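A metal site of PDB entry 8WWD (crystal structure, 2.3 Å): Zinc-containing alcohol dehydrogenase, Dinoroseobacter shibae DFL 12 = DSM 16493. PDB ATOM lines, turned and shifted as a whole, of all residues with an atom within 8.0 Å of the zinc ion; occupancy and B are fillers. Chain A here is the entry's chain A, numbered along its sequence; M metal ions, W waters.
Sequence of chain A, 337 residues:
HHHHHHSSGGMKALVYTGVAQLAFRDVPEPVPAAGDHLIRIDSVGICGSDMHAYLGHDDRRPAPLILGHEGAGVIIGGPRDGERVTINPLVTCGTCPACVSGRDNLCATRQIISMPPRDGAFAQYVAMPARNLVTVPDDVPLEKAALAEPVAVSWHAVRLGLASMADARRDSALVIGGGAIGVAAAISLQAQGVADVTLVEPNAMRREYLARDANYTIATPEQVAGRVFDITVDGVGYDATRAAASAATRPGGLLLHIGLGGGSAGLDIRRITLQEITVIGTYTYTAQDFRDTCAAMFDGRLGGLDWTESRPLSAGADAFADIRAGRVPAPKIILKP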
ATOM      1  N   GLY A  45      -8.460  28.794 -16.042  1.00  0.00           N
ATOM      2  CA  GLY A  45      -8.387  30.064 -15.317  1.00  0.00           C
ATOM      3  C   GLY A  45      -6.960  30.361 -14.856  1.00  0.00           C
ATOM      4  O   GLY A  45      -6.237  29.412 -14.552  1.00  0.00           O
ATOM      5  N   ILE A  46      -6.616  31.646 -14.841  1.00  0.00           N
ATOM      6  CA  ILE A  46      -5.392  32.217 -14.210  1.00  0.00           C
ATOM      7  C   ILE A  46      -5.705  32.552 -12.743  1.00  0.00           C
ATOM      8  O   ILE A  46      -6.620  33.343 -12.489  1.00  0.00           O
ATOM      9  CB  ILE A  46      -4.921  33.473 -14.966  1.00  0.00           C
ATOM     10  CG1 ILE A  46      -4.499  33.205 -16.412  1.00  0.00           C
ATOM     11  CG2 ILE A  46      -3.776  34.147 -14.213  1.00  0.00           C
ATOM     12  CD1 ILE A  46      -4.416  34.460 -17.285  1.00  0.00           C
ATOM     13  N   CYS A  47      -4.946  31.973 -11.812  1.00  0.00           N
ATOM     14  CA  CYS A  47      -5.067  32.144 -10.333  1.00  0.00           C
ATOM     15  C   CYS A  47      -3.956  33.069  -9.786  1.00  0.00           C
ATOM     16  O   CYS A  47      -2.953  33.319 -10.480  1.00  0.00           O
ATOM     17  CB  CYS A  47      -4.874  30.796  -9.651  1.00  0.00           C
ATOM     18  SG  CYS A  47      -5.575  30.712  -8.017  1.00  0.00           S
ATOM     19  N   GLY A  48      -4.107  33.472  -8.524  1.00  0.00           N
ATOM     20  CA  GLY A  48      -3.066  34.186  -7.769  1.00  0.00           C
ATOM     21  C   GLY A  48      -1.790  33.363  -7.638  1.00  0.00           C
ATOM     22  O   GLY A  48      -0.687  33.962  -7.701  1.00  0.00           O
ATOM     23  N   SER A  49      -1.899  32.057  -7.459  1.00  0.00           N
ATOM     24  CA  SER A  49      -0.696  31.191  -7.362  1.00  0.00           C
ATOM     25  C   SER A  49       0.084  31.207  -8.690  1.00  0.00           C
ATOM     26  O   SER A  49       1.331  31.209  -8.639  1.00  0.00           O
ATOM     27  CB  SER A  49      -1.030  29.794  -6.914  1.00  0.00           C
ATOM     28  OG  SER A  49      -1.824  29.103  -7.873  1.00  0.00           O
ATOM     29  N   ASP A  50      -0.581  31.312  -9.835  1.00  0.00           N
ATOM     30  CA  ASP A  50       0.119  31.447 -11.135  1.00  0.00           C
ATOM     31  C   ASP A  50       0.894  32.764 -11.177  1.00  0.00           C
ATOM     32  O   ASP A  50       2.041  32.739 -11.637  1.00  0.00           O
ATOM     33  CB  ASP A  50      -0.842  31.335 -12.327  1.00  0.00           C
ATOM     34  CG  ASP A  50      -1.683  30.070 -12.272  1.00  0.00           C
ATOM     35  OD1 ASP A  50      -1.085  28.991 -12.052  1.00  0.00           O
ATOM     36  OD2 ASP A  50      -2.922  30.218 -12.292  1.00  0.00           O
ATOM     37  N   GLY A  68      -1.142  26.865 -14.051  1.00  0.00           N
ATOM     38  CA  GLY A  68      -2.589  26.710 -14.277  1.00  0.00           C
ATOM     39  C   GLY A  68      -3.133  25.467 -13.571  1.00  0.00           C
ATOM     40  O   GLY A  68      -2.517  24.388 -13.695  1.00  0.00           O
ATOM     41  N   HIS A  69      -4.242  25.578 -12.846  1.00  0.00           N
ATOM     42  CA  HIS A  69      -4.836  24.442 -12.101  1.00  0.00           C
ATOM     43  C   HIS A  69      -6.364  24.519 -12.060  1.00  0.00           C
ATOM     44  O   HIS A  69      -6.955  23.862 -11.204  1.00  0.00           O
ATOM     45  CB  HIS A  69      -4.230  24.385 -10.696  1.00  0.00           C
ATOM     46  CG  HIS A  69      -4.527  25.602  -9.889  1.00  0.00           C
ATOM     47  ND1 HIS A  69      -3.569  26.579  -9.656  1.00  0.00           N
ATOM     48  CD2 HIS A  69      -5.675  26.037  -9.308  1.00  0.00           C
ATOM     49  CE1 HIS A  69      -4.123  27.536  -8.935  1.00  0.00           C
ATOM     50  NE2 HIS A  69      -5.392  27.233  -8.707  1.00  0.00           N
ATOM     51  N   GLU A  70      -6.962  25.310 -12.939  1.00  0.00           N
ATOM     52  CA  GLU A  70      -8.387  25.682 -12.964  1.00  0.00           C
ATOM     53  C   GLU A  70      -8.939  25.331 -14.349  1.00  0.00           C
ATOM     54  O   GLU A  70      -9.355  26.272 -15.074  1.00  0.00           O
ATOM     55  CB  GLU A  70      -8.593  27.184 -12.680  1.00  0.00           C
ATOM     56  CG  GLU A  70      -8.179  27.618 -11.289  1.00  0.00           C
ATOM     57  CD  GLU A  70      -8.361  29.103 -10.950  1.00  0.00           C
ATOM     58  OE1 GLU A  70      -8.792  29.900 -11.861  1.00  0.00           O
ATOM     59  OE2 GLU A  70      -8.080  29.449  -9.789  1.00  0.00           O
ATOM     60  N   PRO A  89      -7.903  19.514  -9.538  1.00  0.00           N
ATOM     61  CA  PRO A  89      -6.481  19.359  -9.740  1.00  0.00           C
ATOM     62  C   PRO A  89      -5.736  18.705  -8.574  1.00  0.00           C
ATOM     63  O   PRO A  89      -4.553  18.453  -8.747  1.00  0.00           O
ATOM     64  CB  PRO A  89      -6.052  20.817  -9.876  1.00  0.00           C
ATOM     65  CG  PRO A  89      -6.934  21.531  -8.882  1.00  0.00           C
ATOM     66  CD  PRO A  89      -8.268  20.867  -9.081  1.00  0.00           C
ATOM     67  N   ILE A 112      -0.849  18.707  -6.475  1.00  0.00           N
ATOM     68  CA  ILE A 112      -1.734  19.578  -7.295  1.00  0.00           C
ATOM     69  C   ILE A 112      -1.098  19.804  -8.664  1.00  0.00           C
ATOM     70  O   ILE A 112       0.116  19.940  -8.777  1.00  0.00           O
ATOM     71  CB  ILE A 112      -2.098  20.878  -6.571  1.00  0.00           C
ATOM     72  CG1 ILE A 112      -3.234  21.595  -7.288  1.00  0.00           C
ATOM     73  CG2 ILE A 112      -0.899  21.798  -6.379  1.00  0.00           C
ATOM     74  CD1 ILE A 112      -3.847  22.687  -6.466  1.00  0.00           C
ATOM     75  N   ALA A 146     -15.088  25.830 -15.805  1.00  0.00           N
ATOM     76  CA  ALA A 146     -13.662  26.058 -15.447  1.00  0.00           C
ATOM     77  C   ALA A 146     -13.599  26.927 -14.178  1.00  0.00           C
ATOM     78  O   ALA A 146     -12.520  27.026 -13.611  1.00  0.00           O
ATOM     79  CB  ALA A 146     -12.901  26.660 -16.583  1.00  0.00           C
ATOM     80  N   GLU A 149     -12.986  25.034  -9.627  1.00  0.00           N
ATOM     81  CA  GLU A 149     -11.860  24.954  -8.649  1.00  0.00           C
ATOM     82  C   GLU A 149     -11.825  26.210  -7.767  1.00  0.00           C
ATOM     83  O   GLU A 149     -11.875  26.072  -6.537  1.00  0.00           O
ATOM     84  CB  GLU A 149     -10.529  24.696  -9.323  1.00  0.00           C
ATOM     85  CG  GLU A 149      -9.446  24.231  -8.356  1.00  0.00           C
ATOM     86  CD  GLU A 149      -8.666  25.342  -7.677  1.00  0.00           C
ATOM     87  OE1 GLU A 149      -8.794  26.491  -8.074  1.00  0.00           O
ATOM     88  OE2 GLU A 149      -7.913  25.040  -6.726  1.00  0.00           O
ATOM     89  N   PRO A 150     -11.751  27.443  -8.319  1.00  0.00           N
ATOM     90  CA  PRO A 150     -11.797  28.645  -7.465  1.00  0.00           C
ATOM     91  C   PRO A 150     -13.121  28.742  -6.693  1.00  0.00           C
ATOM     92  O   PRO A 150     -13.117  29.197  -5.551  1.00  0.00           O
ATOM     93  CB  PRO A 150     -11.597  29.835  -8.421  1.00  0.00           C
ATOM     94  CG  PRO A 150     -11.911  29.281  -9.809  1.00  0.00           C
ATOM     95  CD  PRO A 150     -11.643  27.789  -9.745  1.00  0.00           C
ATOM     96  N   VAL A 151     -14.243  28.259  -7.226  1.00  0.00           N
ATOM     97  CA  VAL A 151     -15.495  28.365  -6.415  1.00  0.00           C
ATOM     98  C   VAL A 151     -15.439  27.296  -5.319  1.00  0.00           C
ATOM     99  O   VAL A 151     -15.962  27.538  -4.223  1.00  0.00           O
ATOM    100  CB  VAL A 151     -16.770  28.326  -7.252  1.00  0.00           C
ATOM    101  CG1 VAL A 151     -18.033  28.403  -6.409  1.00  0.00           C
ATOM    102  CG2 VAL A 151     -16.783  29.460  -8.253  1.00  0.00           C
ATOM    103  N   VAL A 153     -12.840  26.341  -3.651  1.00  0.00           N
ATOM    104  CA  VAL A 153     -11.951  26.848  -2.574  1.00  0.00           C
ATOM    105  C   VAL A 153     -12.837  27.577  -1.560  1.00  0.00           C
ATOM    106  O   VAL A 153     -12.805  27.233  -0.359  1.00  0.00           O
ATOM    107  CB  VAL A 153     -10.818  27.747  -3.109  1.00  0.00           C
ATOM    108  CG1 VAL A 153     -10.092  28.440  -1.970  1.00  0.00           C
ATOM    109  CG2 VAL A 153      -9.816  27.004  -3.988  1.00  0.00           C
ATOM    110  N   ALA A 180     -11.544  36.477  -7.514  1.00  0.00           N
ATOM    111  CA  ALA A 180     -12.280  35.208  -7.680  1.00  0.00           C
ATOM    112  C   ALA A 180     -12.550  34.568  -6.316  1.00  0.00           C
ATOM    113  O   ALA A 180     -13.684  34.048  -6.095  1.00  0.00           O
ATOM    114  CB  ALA A 180     -11.509  34.297  -8.612  1.00  0.00           C
ATOM    115  N   ILE A 181     -11.586  34.592  -5.397  1.00  0.00           N
ATOM    116  CA  ILE A 181     -11.779  33.930  -4.078  1.00  0.00           C
ATOM    117  C   ILE A 181     -12.868  34.664  -3.283  1.00  0.00           C
ATOM    118  O   ILE A 181     -13.640  33.973  -2.622  1.00  0.00           O
ATOM    119  CB  ILE A 181     -10.453  33.834  -3.306  1.00  0.00           C
ATOM    120  CG1 ILE A 181      -9.531  32.818  -3.962  1.00  0.00           C
ATOM    121  CG2 ILE A 181     -10.696  33.501  -1.832  1.00  0.00           C
ATOM    122  CD1 ILE A 181     -10.218  31.458  -4.215  1.00  0.00           C
ATOM    123  N   THR A 284      -7.806  24.475  -0.237  1.00  0.00           N
ATOM    124  CA  THR A 284      -8.530  23.839  -1.347  1.00  0.00           C
ATOM    125  C   THR A 284      -9.904  23.384  -0.843  1.00  0.00           C
ATOM    126  O   THR A 284     -10.686  24.234  -0.429  1.00  0.00           O
ATOM    127  CB  THR A 284      -7.675  22.736  -1.982  1.00  0.00           C
ATOM    128  OG1 THR A 284      -7.182  21.813  -0.997  1.00  0.00           O
ATOM    129  CG2 THR A 284      -6.492  23.299  -2.755  1.00  0.00           C
ATOM    130  N   TYR A 285     -10.173  22.086  -0.920  1.00  0.00           N
ATOM    131  CA  TYR A 285     -11.541  21.504  -0.856  1.00  0.00           C
ATOM    132  C   TYR A 285     -11.386  19.997  -0.692  1.00  0.00           C
ATOM    133  O   TYR A 285     -10.420  19.436  -1.233  1.00  0.00           O
ATOM    134  CB  TYR A 285     -12.306  21.778  -2.149  1.00  0.00           C
ATOM    135  CG  TYR A 285     -11.353  21.883  -3.308  1.00  0.00           C
ATOM    136  CD1 TYR A 285     -10.772  20.764  -3.855  1.00  0.00           C
ATOM    137  CD2 TYR A 285     -10.929  23.140  -3.762  1.00  0.00           C
ATOM    138  CE1 TYR A 285      -9.836  20.879  -4.870  1.00  0.00           C
ATOM    139  CE2 TYR A 285      -9.999  23.263  -4.772  1.00  0.00           C
ATOM    140  CZ  TYR A 285      -9.442  22.126  -5.325  1.00  0.00           C
ATOM    141  OH  TYR A 285      -8.491  22.220  -6.286  1.00  0.00           O
ATOM    142  N   LYS A 332     -11.617  37.112 -13.189  1.00  0.00           N
ATOM    143  CA  LYS A 332     -11.064  35.818 -13.664  1.00  0.00           C
ATOM    144  C   LYS A 332     -10.857  35.918 -15.173  1.00  0.00           C
ATOM    145  O   LYS A 332     -11.831  36.249 -15.919  1.00  0.00           O
ATOM    146  CB  LYS A 332     -12.000  34.674 -13.260  1.00  0.00           C
ATOM    147  CG  LYS A 332     -11.575  33.282 -13.689  1.00  0.00           C
ATOM    148  CD  LYS A 332     -10.222  32.871 -13.128  1.00  0.00           C
ATOM    149  CE  LYS A 332     -10.120  32.951 -11.615  1.00  0.00           C
ATOM    150  NZ  LYS A 332      -8.868  32.324 -11.130  1.00  0.00           N
HETATM  151 ZN    ZN M   1      -6.969  28.705  -8.187  1.00  0.00          ZN
HETATM  152  O   HOH W   1      -8.414  29.737  -6.110  1.00  0.00           O
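Glu 149 touches the zinc ion.
Of the 21 residues printed, 4 come within 4 Å of the zinc ion.
The nearest printed residue that does not touch the zinc ion is Pro 150 (4.8 Å).
The side-chain carboxylate (OD2) of Asp 50 sits at hydrogen-bond distance from the backbone NH (N) of Cys 47 (2.7 Å).
The side-chain amino group (NZ) of Lys 332 lies within salt-bridge range of the side-chain carboxylate (OE1) of Glu 70 (2.5 Å).
OH of Tyr 285 sits at hydrogen-bond distance from OE2 of Glu 149, 2.9 Å away.
O of Glu 70 lies within hydrogen-bond range of N of Gly 45, at 2.8 Å.
The side-chain carboxylate (OE2) of Glu 70 is bound to the zinc ion, 2.1 Å away.
The zinc ion is bound by NE2 of His 69, at 2.2 Å.
The zinc ion is bound by SG of Cys 47.
The zinc ion has three donor atoms within binding distance.
Slightly farther from the zinc ion lies water W1 (2.7 Å).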
